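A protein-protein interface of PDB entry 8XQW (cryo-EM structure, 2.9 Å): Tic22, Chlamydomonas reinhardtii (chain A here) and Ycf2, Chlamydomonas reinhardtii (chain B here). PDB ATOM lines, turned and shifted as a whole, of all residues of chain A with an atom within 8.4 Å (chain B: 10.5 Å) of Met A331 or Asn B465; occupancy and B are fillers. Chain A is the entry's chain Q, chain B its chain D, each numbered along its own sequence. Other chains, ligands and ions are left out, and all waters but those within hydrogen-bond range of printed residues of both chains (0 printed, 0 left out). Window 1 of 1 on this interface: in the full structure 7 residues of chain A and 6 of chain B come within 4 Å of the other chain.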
ATOM      1  N   MET A  96      28.638  -7.489  21.305  1.00  0.00           N
ATOM      2  CA  MET A  96      29.946  -7.773  20.728  1.00  0.00           C
ATOM      3  C   MET A  96      30.309  -6.747  19.660  1.00  0.00           C
ATOM      4  O   MET A  96      29.478  -6.375  18.837  1.00  0.00           O
ATOM      5  CB  MET A  96      29.974  -9.184  20.139  1.00  0.00           C
ATOM      6  CG  MET A  96      31.290  -9.551  19.499  1.00  0.00           C
ATOM      7  SD  MET A  96      31.967 -11.095  20.127  1.00  0.00           S
ATOM      8  CE  MET A  96      30.931 -12.286  19.294  1.00  0.00           C
ATOM      9  N   VAL A 101      32.850 -10.046  15.530  1.00  0.00           N
ATOM     10  CA  VAL A 101      31.881 -10.816  14.761  1.00  0.00           C
ATOM     11  C   VAL A 101      32.432 -11.121  13.380  1.00  0.00           C
ATOM     12  O   VAL A 101      32.342 -12.255  12.894  1.00  0.00           O
ATOM     13  CB  VAL A 101      30.540 -10.067  14.673  1.00  0.00           C
ATOM     14  CG1 VAL A 101      29.445 -11.020  14.258  1.00  0.00           C
ATOM     15  CG2 VAL A 101      30.206  -9.425  15.996  1.00  0.00           C
ATOM     16  N   TYR A 170      28.582  -9.862   5.444  1.00  0.00           N
ATOM     17  CA  TYR A 170      28.106  -9.266   6.685  1.00  0.00           C
ATOM     18  C   TYR A 170      28.327  -7.764   6.664  1.00  0.00           C
ATOM     19  O   TYR A 170      27.448  -6.988   7.049  1.00  0.00           O
ATOM     20  CB  TYR A 170      28.805  -9.889   7.892  1.00  0.00           C
ATOM     21  CG  TYR A 170      28.561  -9.123   9.175  1.00  0.00           C
ATOM     22  CD1 TYR A 170      27.413  -9.334   9.921  1.00  0.00           C
ATOM     23  CD2 TYR A 170      29.469  -8.177   9.631  1.00  0.00           C
ATOM     24  CE1 TYR A 170      27.178  -8.631  11.085  1.00  0.00           C
ATOM     25  CE2 TYR A 170      29.241  -7.470  10.793  1.00  0.00           C
ATOM     26  CZ  TYR A 170      28.095  -7.700  11.515  1.00  0.00           C
ATOM     27  OH  TYR A 170      27.866  -7.000  12.673  1.00  0.00           O
ATOM     28  N   THR A 174      25.261  -4.588   7.076  1.00  0.00           N
ATOM     29  CA  THR A 174      25.174  -3.572   8.123  1.00  0.00           C
ATOM     30  C   THR A 174      26.014  -2.348   7.762  1.00  0.00           C
ATOM     31  O   THR A 174      26.984  -1.993   8.426  1.00  0.00           O
ATOM     32  CB  THR A 174      25.603  -4.165   9.459  1.00  0.00           C
ATOM     33  OG1 THR A 174      25.868  -3.107  10.387  1.00  0.00           O
ATOM     34  CG2 THR A 174      26.858  -5.001   9.283  1.00  0.00           C
ATOM     35  N   ILE A 214      12.581 -21.126   8.760  1.00  0.00           N
ATOM     36  CA  ILE A 214      13.051 -19.765   8.551  1.00  0.00           C
ATOM     37  C   ILE A 214      14.570 -19.785   8.642  1.00  0.00           C
ATOM     38  O   ILE A 214      15.137 -20.281   9.624  1.00  0.00           O
ATOM     39  CB  ILE A 214      12.440 -18.792   9.563  1.00  0.00           C
ATOM     40  CG1 ILE A 214      10.923 -18.742   9.384  1.00  0.00           C
ATOM     41  CG2 ILE A 214      13.047 -17.413   9.402  1.00  0.00           C
ATOM     42  CD1 ILE A 214      10.208 -17.949  10.444  1.00  0.00           C
ATOM     43  N   SER A 325      18.436 -21.031  13.325  1.00  0.00           N
ATOM     44  CA  SER A 325      18.534 -20.203  12.133  1.00  0.00           C
ATOM     45  C   SER A 325      19.790 -19.342  12.188  1.00  0.00           C
ATOM     46  O   SER A 325      20.131 -18.770  13.222  1.00  0.00           O
ATOM     47  CB  SER A 325      17.303 -19.308  11.984  1.00  0.00           C
ATOM     48  OG  SER A 325      16.123 -19.997  12.353  1.00  0.00           O
ATOM     49  N   PHE A 326      20.466 -19.245  11.044  1.00  0.00           N
ATOM     50  CA  PHE A 326      21.714 -18.492  10.976  1.00  0.00           C
ATOM     51  C   PHE A 326      21.496 -17.010  11.252  1.00  0.00           C
ATOM     52  O   PHE A 326      22.281 -16.385  11.976  1.00  0.00           O
ATOM     53  CB  PHE A 326      22.349 -18.693   9.605  1.00  0.00           C
ATOM     54  CG  PHE A 326      23.783 -18.295   9.540  1.00  0.00           C
ATOM     55  CD1 PHE A 326      24.773 -19.169   9.943  1.00  0.00           C
ATOM     56  CD2 PHE A 326      24.145 -17.048   9.070  1.00  0.00           C
ATOM     57  CE1 PHE A 326      26.100 -18.806   9.882  1.00  0.00           C
ATOM     58  CE2 PHE A 326      25.470 -16.678   9.007  1.00  0.00           C
ATOM     59  CZ  PHE A 326      26.450 -17.558   9.415  1.00  0.00           C
ATOM     60  N   GLU A 327      20.439 -16.429  10.681  1.00  0.00           N
ATOM     61  CA  GLU A 327      20.190 -15.001  10.844  1.00  0.00           C
ATOM     62  C   GLU A 327      19.949 -14.647  12.304  1.00  0.00           C
ATOM     63  O   GLU A 327      20.462 -13.641  12.803  1.00  0.00           O
ATOM     64  CB  GLU A 327      18.995 -14.574   9.991  1.00  0.00           C
ATOM     65  CG  GLU A 327      19.134 -14.877   8.513  1.00  0.00           C
ATOM     66  CD  GLU A 327      18.736 -16.295   8.170  1.00  0.00           C
ATOM     67  OE1 GLU A 327      18.676 -16.627   6.969  1.00  0.00           O
ATOM     68  OE2 GLU A 327      18.490 -17.082   9.106  1.00  0.00           O
ATOM     69  N   GLU A 328      19.160 -15.463  13.003  1.00  0.00           N
ATOM     70  CA  GLU A 328      18.947 -15.229  14.426  1.00  0.00           C
ATOM     71  C   GLU A 328      20.249 -15.351  15.205  1.00  0.00           C
ATOM     72  O   GLU A 328      20.508 -14.555  16.116  1.00  0.00           O
ATOM     73  CB  GLU A 328      17.906 -16.209  14.964  1.00  0.00           C
ATOM     74  CG  GLU A 328      16.525 -15.613  15.175  1.00  0.00           C
ATOM     75  CD  GLU A 328      16.518 -14.500  16.201  1.00  0.00           C
ATOM     76  OE1 GLU A 328      16.322 -14.795  17.399  1.00  0.00           O
ATOM     77  OE2 GLU A 328      16.705 -13.330  15.811  1.00  0.00           O
ATOM     78  N   VAL A 329      21.081 -16.331  14.851  1.00  0.00           N
ATOM     79  CA  VAL A 329      22.366 -16.504  15.524  1.00  0.00           C
ATOM     80  C   VAL A 329      23.210 -15.248  15.384  1.00  0.00           C
ATOM     81  O   VAL A 329      23.757 -14.738  16.365  1.00  0.00           O
ATOM     82  CB  VAL A 329      23.102 -17.740  14.976  1.00  0.00           C
ATOM     83  CG1 VAL A 329      24.601 -17.582  15.142  1.00  0.00           C
ATOM     84  CG2 VAL A 329      22.624 -18.989  15.681  1.00  0.00           C
ATOM     85  N   VAL A 330      23.319 -14.716  14.166  1.00  0.00           N
ATOM     86  CA  VAL A 330      24.176 -13.548  13.993  1.00  0.00           C
ATOM     87  C   VAL A 330      23.543 -12.306  14.607  1.00  0.00           C
ATOM     88  O   VAL A 330      24.254 -11.435  15.121  1.00  0.00           O
ATOM     89  CB  VAL A 330      24.536 -13.337  12.511  1.00  0.00           C
ATOM     90  CG1 VAL A 330      25.084 -14.617  11.920  1.00  0.00           C
ATOM     91  CG2 VAL A 330      23.340 -12.859  11.721  1.00  0.00           C
ATOM     92  N   MET A 331      22.212 -12.205  14.601  1.00  0.00           N
ATOM     93  CA  MET A 331      21.580 -11.052  15.227  1.00  0.00           C
ATOM     94  C   MET A 331      21.809 -11.059  16.731  1.00  0.00           C
ATOM     95  O   MET A 331      21.981 -10.000  17.344  1.00  0.00           O
ATOM     96  CB  MET A 331      20.088 -11.027  14.910  1.00  0.00           C
ATOM     97  CG  MET A 331      19.714 -10.104  13.764  1.00  0.00           C
ATOM     98  SD  MET A 331      17.956 -10.170  13.361  1.00  0.00           S
ATOM     99  CE  MET A 331      17.795 -11.862  12.798  1.00  0.00           C
ATOM    100  N   ARG A 332      21.821 -12.243  17.343  1.00  0.00           N
ATOM    101  CA  ARG A 332      22.142 -12.321  18.763  1.00  0.00           C
ATOM    102  C   ARG A 332      23.628 -12.092  19.001  1.00  0.00           C
ATOM    103  O   ARG A 332      24.015 -11.506  20.016  1.00  0.00           O
ATOM    104  CB  ARG A 332      21.715 -13.672  19.330  1.00  0.00           C
ATOM    105  CG  ARG A 332      20.230 -13.951  19.229  1.00  0.00           C
ATOM    106  CD  ARG A 332      19.734 -14.689  20.456  1.00  0.00           C
ATOM    107  NE  ARG A 332      18.695 -15.664  20.137  1.00  0.00           N
ATOM    108  CZ  ARG A 332      18.914 -16.967  19.982  1.00  0.00           C
ATOM    109  NH1 ARG A 332      20.135 -17.456  20.113  1.00  0.00           N
ATOM    110  NH2 ARG A 332      17.908 -17.780  19.696  1.00  0.00           N
ATOM    111  N   MET A 333      24.472 -12.552  18.079  1.00  0.00           N
ATOM    112  CA  MET A 333      25.909 -12.376  18.236  1.00  0.00           C
ATOM    113  C   MET A 333      26.283 -10.903  18.235  1.00  0.00           C
ATOM    114  O   MET A 333      27.087 -10.461  19.062  1.00  0.00           O
ATOM    115  CB  MET A 333      26.643 -13.111  17.117  1.00  0.00           C
ATOM    116  CG  MET A 333      27.989 -13.672  17.500  1.00  0.00           C
ATOM    117  SD  MET A 333      28.669 -14.689  16.180  1.00  0.00           S
ATOM    118  CE  MET A 333      29.957 -15.566  17.055  1.00  0.00           C
ATOM    119  N   THR A 334      25.703 -10.127  17.322  1.00  0.00           N
ATOM    120  CA  THR A 334      26.059  -8.716  17.221  1.00  0.00           C
ATOM    121  C   THR A 334      25.622  -7.941  18.459  1.00  0.00           C
ATOM    122  O   THR A 334      26.440  -7.290  19.116  1.00  0.00           O
ATOM    123  CB  THR A 334      25.455  -8.107  15.958  1.00  0.00           C
ATOM    124  OG1 THR A 334      24.026  -8.114  16.060  1.00  0.00           O
ATOM    125  CG2 THR A 334      25.896  -8.877  14.725  1.00  0.00           C
ATOM    126  N   ALA A 335      24.338  -7.990  18.792  1.00  0.00           N
ATOM    127  CA  ALA A 335      23.825  -7.232  19.932  1.00  0.00           C
ATOM    128  C   ALA A 335      23.915  -8.027  21.230  1.00  0.00           C
ATOM    129  O   ALA A 335      22.935  -8.177  21.956  1.00  0.00           O
ATOM    130  CB  ALA A 335      22.393  -6.793  19.662  1.00  0.00           C
ATOM    131  N   SER A 336      25.104  -8.529  21.537  1.00  0.00           N
ATOM    132  CA  SER A 336      25.340  -9.318  22.736  1.00  0.00           C
ATOM    133  C   SER A 336      26.193  -8.535  23.726  1.00  0.00           C
ATOM    134  O   SER A 336      27.043  -7.731  23.337  1.00  0.00           O
ATOM    135  CB  SER A 336      26.031 -10.639  22.394  1.00  0.00           C
ATOM    136  OG  SER A 336      25.657 -11.655  23.302  1.00  0.00           O
ATOM    137  N   TRP A 344      28.970 -16.415  23.660  1.00  0.00           N
ATOM    138  CA  TRP A 344      29.224 -16.252  22.235  1.00  0.00           C
ATOM    139  C   TRP A 344      30.704 -16.153  21.917  1.00  0.00           C
ATOM    140  O   TRP A 344      31.112 -16.512  20.811  1.00  0.00           O
ATOM    141  CB  TRP A 344      28.518 -15.003  21.711  1.00  0.00           C
ATOM    142  CG  TRP A 344      27.042 -15.152  21.584  1.00  0.00           C
ATOM    143  CD1 TRP A 344      26.089 -14.422  22.220  1.00  0.00           C
ATOM    144  CD2 TRP A 344      26.348 -16.092  20.763  1.00  0.00           C
ATOM    145  NE1 TRP A 344      24.842 -14.847  21.850  1.00  0.00           N
ATOM    146  CE2 TRP A 344      24.974 -15.873  20.954  1.00  0.00           C
ATOM    147  CE3 TRP A 344      26.756 -17.097  19.885  1.00  0.00           C
ATOM    148  CZ2 TRP A 344      24.005 -16.622  20.302  1.00  0.00           C
ATOM    149  CZ3 TRP A 344      25.798 -17.838  19.240  1.00  0.00           C
ATOM    150  CH2 TRP A 344      24.435 -17.597  19.449  1.00  0.00           C
ATOM    151  N   ASN B 457      25.935   5.212  11.767  1.00  0.00           N
ATOM    152  CA  ASN B 457      25.605   3.907  11.207  1.00  0.00           C
ATOM    153  C   ASN B 457      25.487   2.858  12.303  1.00  0.00           C
ATOM    154  O   ASN B 457      24.473   2.156  12.404  1.00  0.00           O
ATOM    155  CB  ASN B 457      26.657   3.484  10.186  1.00  0.00           C
ATOM    156  CG  ASN B 457      26.833   4.492   9.079  1.00  0.00           C
ATOM    157  OD1 ASN B 457      27.948   4.741   8.625  1.00  0.00           O
ATOM    158  ND2 ASN B 457      25.732   5.084   8.642  1.00  0.00           N
ATOM    159  N   ASN B 458      26.521   2.744  13.141  1.00  0.00           N
ATOM    160  CA  ASN B 458      26.516   1.716  14.175  1.00  0.00           C
ATOM    161  C   ASN B 458      25.416   1.960  15.197  1.00  0.00           C
ATOM    162  O   ASN B 458      24.809   1.009  15.701  1.00  0.00           O
ATOM    163  CB  ASN B 458      27.878   1.652  14.857  1.00  0.00           C
ATOM    164  CG  ASN B 458      28.906   0.928  14.023  1.00  0.00           C
ATOM    165  OD1 ASN B 458      29.071  -0.284  14.139  1.00  0.00           O
ATOM    166  ND2 ASN B 458      29.602   1.669  13.172  1.00  0.00           N
ATOM    167  N   LEU B 459      25.133   3.223  15.508  1.00  0.00           N
ATOM    168  CA  LEU B 459      24.080   3.517  16.471  1.00  0.00           C
ATOM    169  C   LEU B 459      22.723   3.087  15.941  1.00  0.00           C
ATOM    170  O   LEU B 459      21.928   2.473  16.668  1.00  0.00           O
ATOM    171  CB  LEU B 459      24.079   5.007  16.805  1.00  0.00           C
ATOM    172  CG  LEU B 459      23.141   5.455  17.924  1.00  0.00           C
ATOM    173  CD1 LEU B 459      23.250   4.520  19.111  1.00  0.00           C
ATOM    174  CD2 LEU B 459      23.463   6.876  18.338  1.00  0.00           C
ATOM    175  N   TYR B 460      22.435   3.405  14.679  1.00  0.00           N
ATOM    176  CA  TYR B 460      21.169   2.982  14.095  1.00  0.00           C
ATOM    177  C   TYR B 460      21.074   1.464  14.050  1.00  0.00           C
ATOM    178  O   TYR B 460      20.019   0.891  14.342  1.00  0.00           O
ATOM    179  CB  TYR B 460      21.005   3.570  12.698  1.00  0.00           C
ATOM    180  CG  TYR B 460      19.787   3.037  11.987  1.00  0.00           C
ATOM    181  CD1 TYR B 460      18.512   3.443  12.359  1.00  0.00           C
ATOM    182  CD2 TYR B 460      19.907   2.119  10.954  1.00  0.00           C
ATOM    183  CE1 TYR B 460      17.395   2.956  11.714  1.00  0.00           C
ATOM    184  CE2 TYR B 460      18.799   1.626  10.307  1.00  0.00           C
ATOM    185  CZ  TYR B 460      17.545   2.046  10.692  1.00  0.00           C
ATOM    186  OH  TYR B 460      16.434   1.555  10.045  1.00  0.00           O
ATOM    187  N   ASN B 461      22.166   0.795  13.672  1.00  0.00           N
ATOM    188  CA  ASN B 461      22.158  -0.664  13.666  1.00  0.00           C
ATOM    189  C   ASN B 461      21.864  -1.207  15.055  1.00  0.00           C
ATOM    190  O   ASN B 461      21.109  -2.169  15.214  1.00  0.00           O
ATOM    191  CB  ASN B 461      23.494  -1.201  13.157  1.00  0.00           C
ATOM    192  CG  ASN B 461      23.859  -0.651  11.805  1.00  0.00           C
ATOM    193  OD1 ASN B 461      25.035  -0.495  11.482  1.00  0.00           O
ATOM    194  ND2 ASN B 461      22.849  -0.338  11.003  1.00  0.00           N
ATOM    195  N   TYR B 462      22.453  -0.585  16.075  1.00  0.00           N
ATOM    196  CA  TYR B 462      22.233  -1.002  17.453  1.00  0.00           C
ATOM    197  C   TYR B 462      20.758  -0.911  17.824  1.00  0.00           C
ATOM    198  O   TYR B 462      20.143  -1.898  18.260  1.00  0.00           O
ATOM    199  CB  TYR B 462      23.082  -0.120  18.367  1.00  0.00           C
ATOM    200  CG  TYR B 462      23.238  -0.601  19.778  1.00  0.00           C
ATOM    201  CD1 TYR B 462      23.883  -1.791  20.055  1.00  0.00           C
ATOM    202  CD2 TYR B 462      22.763   0.152  20.837  1.00  0.00           C
ATOM    203  CE1 TYR B 462      24.041  -2.224  21.346  1.00  0.00           C
ATOM    204  CE2 TYR B 462      22.910  -0.274  22.131  1.00  0.00           C
ATOM    205  CZ  TYR B 462      23.549  -1.463  22.382  1.00  0.00           C
ATOM    206  OH  TYR B 462      23.701  -1.897  23.678  1.00  0.00           O
ATOM    207  N   ILE B 463      20.177   0.278  17.647  1.00  0.00           N
ATOM    208  CA  ILE B 463      18.768   0.480  17.973  1.00  0.00           C
ATOM    209  C   ILE B 463      17.900  -0.520  17.221  1.00  0.00           C
ATOM    210  O   ILE B 463      17.037  -1.184  17.807  1.00  0.00           O
ATOM    211  CB  ILE B 463      18.342   1.926  17.657  1.00  0.00           C
ATOM    212  CG1 ILE B 463      19.273   2.932  18.338  1.00  0.00           C
ATOM    213  CG2 ILE B 463      16.903   2.150  18.072  1.00  0.00           C
ATOM    214  CD1 ILE B 463      19.285   2.844  19.843  1.00  0.00           C
ATOM    215  N   SER B 464      18.121  -0.645  15.910  1.00  0.00           N
ATOM    216  CA  SER B 464      17.249  -1.473  15.090  1.00  0.00           C
ATOM    217  C   SER B 464      17.363  -2.944  15.462  1.00  0.00           C
ATOM    218  O   SER B 464      16.348  -3.643  15.557  1.00  0.00           O
ATOM    219  CB  SER B 464      17.567  -1.264  13.612  1.00  0.00           C
ATOM    220  OG  SER B 464      17.745   0.110  13.316  1.00  0.00           O
ATOM    221  N   ASN B 465      18.585  -3.436  15.673  1.00  0.00           N
ATOM    222  CA  ASN B 465      18.759  -4.837  16.032  1.00  0.00           C
ATOM    223  C   ASN B 465      18.088  -5.145  17.360  1.00  0.00           C
ATOM    224  O   ASN B 465      17.431  -6.184  17.504  1.00  0.00           O
ATOM    225  CB  ASN B 465      20.244  -5.188  16.090  1.00  0.00           C
ATOM    226  CG  ASN B 465      20.496  -6.659  15.843  1.00  0.00           C
ATOM    227  OD1 ASN B 465      19.672  -7.504  16.192  1.00  0.00           O
ATOM    228  ND2 ASN B 465      21.630  -6.976  15.233  1.00  0.00           N
ATOM    229  N   LYS B 466      18.220  -4.247  18.340  1.00  0.00           N
ATOM    230  CA  LYS B 466      17.594  -4.517  19.628  1.00  0.00           C
ATOM    231  C   LYS B 466      16.074  -4.458  19.542  1.00  0.00           C
ATOM    232  O   LYS B 466      15.385  -5.280  20.150  1.00  0.00           O
ATOM    233  CB  LYS B 466      18.126  -3.572  20.699  1.00  0.00           C
ATOM    234  CG  LYS B 466      19.194  -4.249  21.518  1.00  0.00           C
ATOM    235  CD  LYS B 466      20.341  -3.360  21.901  1.00  0.00           C
ATOM    236  CE  LYS B 466      21.531  -4.241  22.259  1.00  0.00           C
ATOM    237  NZ  LYS B 466      22.173  -3.857  23.551  1.00  0.00           N
ATOM    238  N   THR B 467      15.530  -3.502  18.789  1.00  0.00           N
ATOM    239  CA  THR B 467      14.077  -3.469  18.638  1.00  0.00           C
ATOM    240  C   THR B 467      13.570  -4.723  17.939  1.00  0.00           C
ATOM    241  O   THR B 467      12.554  -5.302  18.345  1.00  0.00           O
ATOM    242  CB  THR B 467      13.641  -2.227  17.865  1.00  0.00           C
ATOM    243  OG1 THR B 467      14.255  -2.230  16.570  1.00  0.00           O
ATOM    244  CG2 THR B 467      14.019  -0.964  18.618  1.00  0.00           C
ATOM    245  N   ALA B 468      14.269  -5.163  16.892  1.00  0.00           N
ATOM    246  CA  ALA B 468      13.841  -6.351  16.171  1.00  0.00           C
ATOM    247  C   ALA B 468      13.874  -7.574  17.074  1.00  0.00           C
ATOM    248  O   ALA B 468      12.912  -8.350  17.122  1.00  0.00           O
ATOM    249  CB  ALA B 468      14.720  -6.563  14.936  1.00  0.00           C
ATOM    250  N   LEU B 469      14.965  -7.746  17.824  1.00  0.00           N
ATOM    251  CA  LEU B 469      15.062  -8.900  18.707  1.00  0.00           C
ATOM    252  C   LEU B 469      14.039  -8.821  19.831  1.00  0.00           C
ATOM    253  O   LEU B 469      13.499  -9.847  20.259  1.00  0.00           O
ATOM    254  CB  LEU B 469      16.477  -9.021  19.266  1.00  0.00           C
ATOM    255  CG  LEU B 469      16.978 -10.460  19.398  1.00  0.00           C
ATOM    256  CD1 LEU B 469      16.386 -11.323  18.307  1.00  0.00           C
ATOM    257  CD2 LEU B 469      18.492 -10.501  19.334  1.00  0.00           C
ATOM    258  N   SER B 470      13.739  -7.613  20.309  1.00  0.00           N
ATOM    259  CA  SER B 470      12.722  -7.470  21.343  1.00  0.00           C
ATOM    260  C   SER B 470      11.368  -7.936  20.837  1.00  0.00           C
ATOM    261  O   SER B 470      10.703  -8.764  21.477  1.00  0.00           O
ATOM    262  CB  SER B 470      12.646  -6.019  21.811  1.00  0.00           C
ATOM    263  OG  SER B 470      11.328  -5.691  22.212  1.00  0.00           O
ATOM    264  N   THR B 471      10.935  -7.399  19.691  1.00  0.00           N
ATOM    265  CA  THR B 471       9.672  -7.845  19.112  1.00  0.00           C
ATOM    266  C   THR B 471       9.662  -9.352  18.915  1.00  0.00           C
ATOM    267  O   THR B 471       8.700 -10.024  19.302  1.00  0.00           O
ATOM    268  CB  THR B 471       9.402  -7.147  17.779  1.00  0.00           C
ATOM    269  OG1 THR B 471      10.250  -7.703  16.766  1.00  0.00           O
ATOM    270  CG2 THR B 471       9.612  -5.650  17.886  1.00  0.00           C
ATOM    271  N   LYS B 472      10.735  -9.905  18.346  1.00  0.00           N
ATOM    272  CA  LYS B 472      10.744 -11.328  18.029  1.00  0.00           C
ATOM    273  C   LYS B 472      10.628 -12.178  19.288  1.00  0.00           C
ATOM    274  O   LYS B 472       9.811 -13.103  19.346  1.00  0.00           O
ATOM    275  CB  LYS B 472      12.007 -11.683  17.250  1.00  0.00           C
ATOM    276  CG  LYS B 472      11.914 -12.979  16.459  1.00  0.00           C
ATOM    277  CD  LYS B 472      12.247 -14.181  17.324  1.00  0.00           C
ATOM    278  CE  LYS B 472      12.720 -15.356  16.497  1.00  0.00           C
ATOM    279  NZ  LYS B 472      13.546 -16.272  17.323  1.00  0.00           N
ATOM    280  N   ASN B 473      11.433 -11.882  20.310  1.00  0.00           N
ATOM    281  CA  ASN B 473      11.420 -12.711  21.511  1.00  0.00           C
ATOM    282  C   ASN B 473      10.111 -12.574  22.278  1.00  0.00           C
ATOM    283  O   ASN B 473       9.555 -13.571  22.756  1.00  0.00           O
ATOM    284  CB  ASN B 473      12.612 -12.372  22.404  1.00  0.00           C
ATOM    285  CG  ASN B 473      13.928 -12.769  21.782  1.00  0.00           C
ATOM    286  OD1 ASN B 473      14.249 -12.366  20.667  1.00  0.00           O
ATOM    287  ND2 ASN B 473      14.694 -13.581  22.497  1.00  0.00           N
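Hydrophobic or aromatic side chains of chain B that line the printed part of chain A: Leu B469.
Among the printed residues, 7 pairs touch across the chains.
Among the printed residues, Asp or Glu carboxylates within 4 Å of a Lys or Arg side-chain nitrogen of the other chain: Glu A328 with Lys B472 (3.1 Å).
The side-chain amide oxygen (OD1) of Asn B461 is in hydrogen-bond range of the side-chain hydroxyl (OG1) of Thr A174.
OG1 of Thr A334 is in hydrogen-bond range of ND2 of Asn B465 (2.8 Å).
The side-chain amino group (NZ) of Lys B472 lies within salt-bridge range of the side-chain carboxylate (OE1) of Glu A328, at 3.1 Å.
Met A331 touches just one residue of chain B: Asn B465.
Asn B465 touches just these residues of chain A: Met A331 (3.6 Å) and Thr A334 (2.8 Å).
No residue of chain B comes within 4 Å of Val A330.
No residue of chain A comes within 4 Å of Ser B464.
Of the printed residues of chain A, Asn B461 touches Thr A174.
Printed residues of chain A within 4 Å of Leu B469: Glu A328 (3.2 Å) and Arg A332 (3.9 Å).
Met A96 touches none of the printed residues of chain B.
The nearest printed residue of chain A that does not touch Lys B472 is Arg A332 (5.2 Å).
N of Met A96 sits at hydrogen-bond distance from O of Thr A334, 3.1 Å away.
The side-chain hydroxyl of Thr A334 is in hydrogen-bond range of the backbone carbonyl oxygen of Met A331 (3.1 Å).
The side-chain amino group (NZ) of Lys B466 sits at hydrogen-bond distance from the side-chain hydroxyl (OH) of Tyr B462 (2.5 Å).
The side-chain carboxylate (OE1) of Glu A328 is in salt-bridge range of the guanidinium group (NE) of Arg A332 (3.7 Å).
The backbone carbonyl oxygen of Leu B469 lies close to the side-chain amide oxygen of Asn B473, at 2.7 Å.
The side-chain amide oxygen of Asn B461 lies close to the backbone carbonyl oxygen of Asn B457.
Among the printed residues, merely in contact across the chains: Glu A328 with Leu B469 (3.2 Å), Met A331 with Asn B465 (3.6 Å), Arg A332 with Leu B469 (3.9 Å) and Ala A335 with Lys B466 (3.7 Å).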
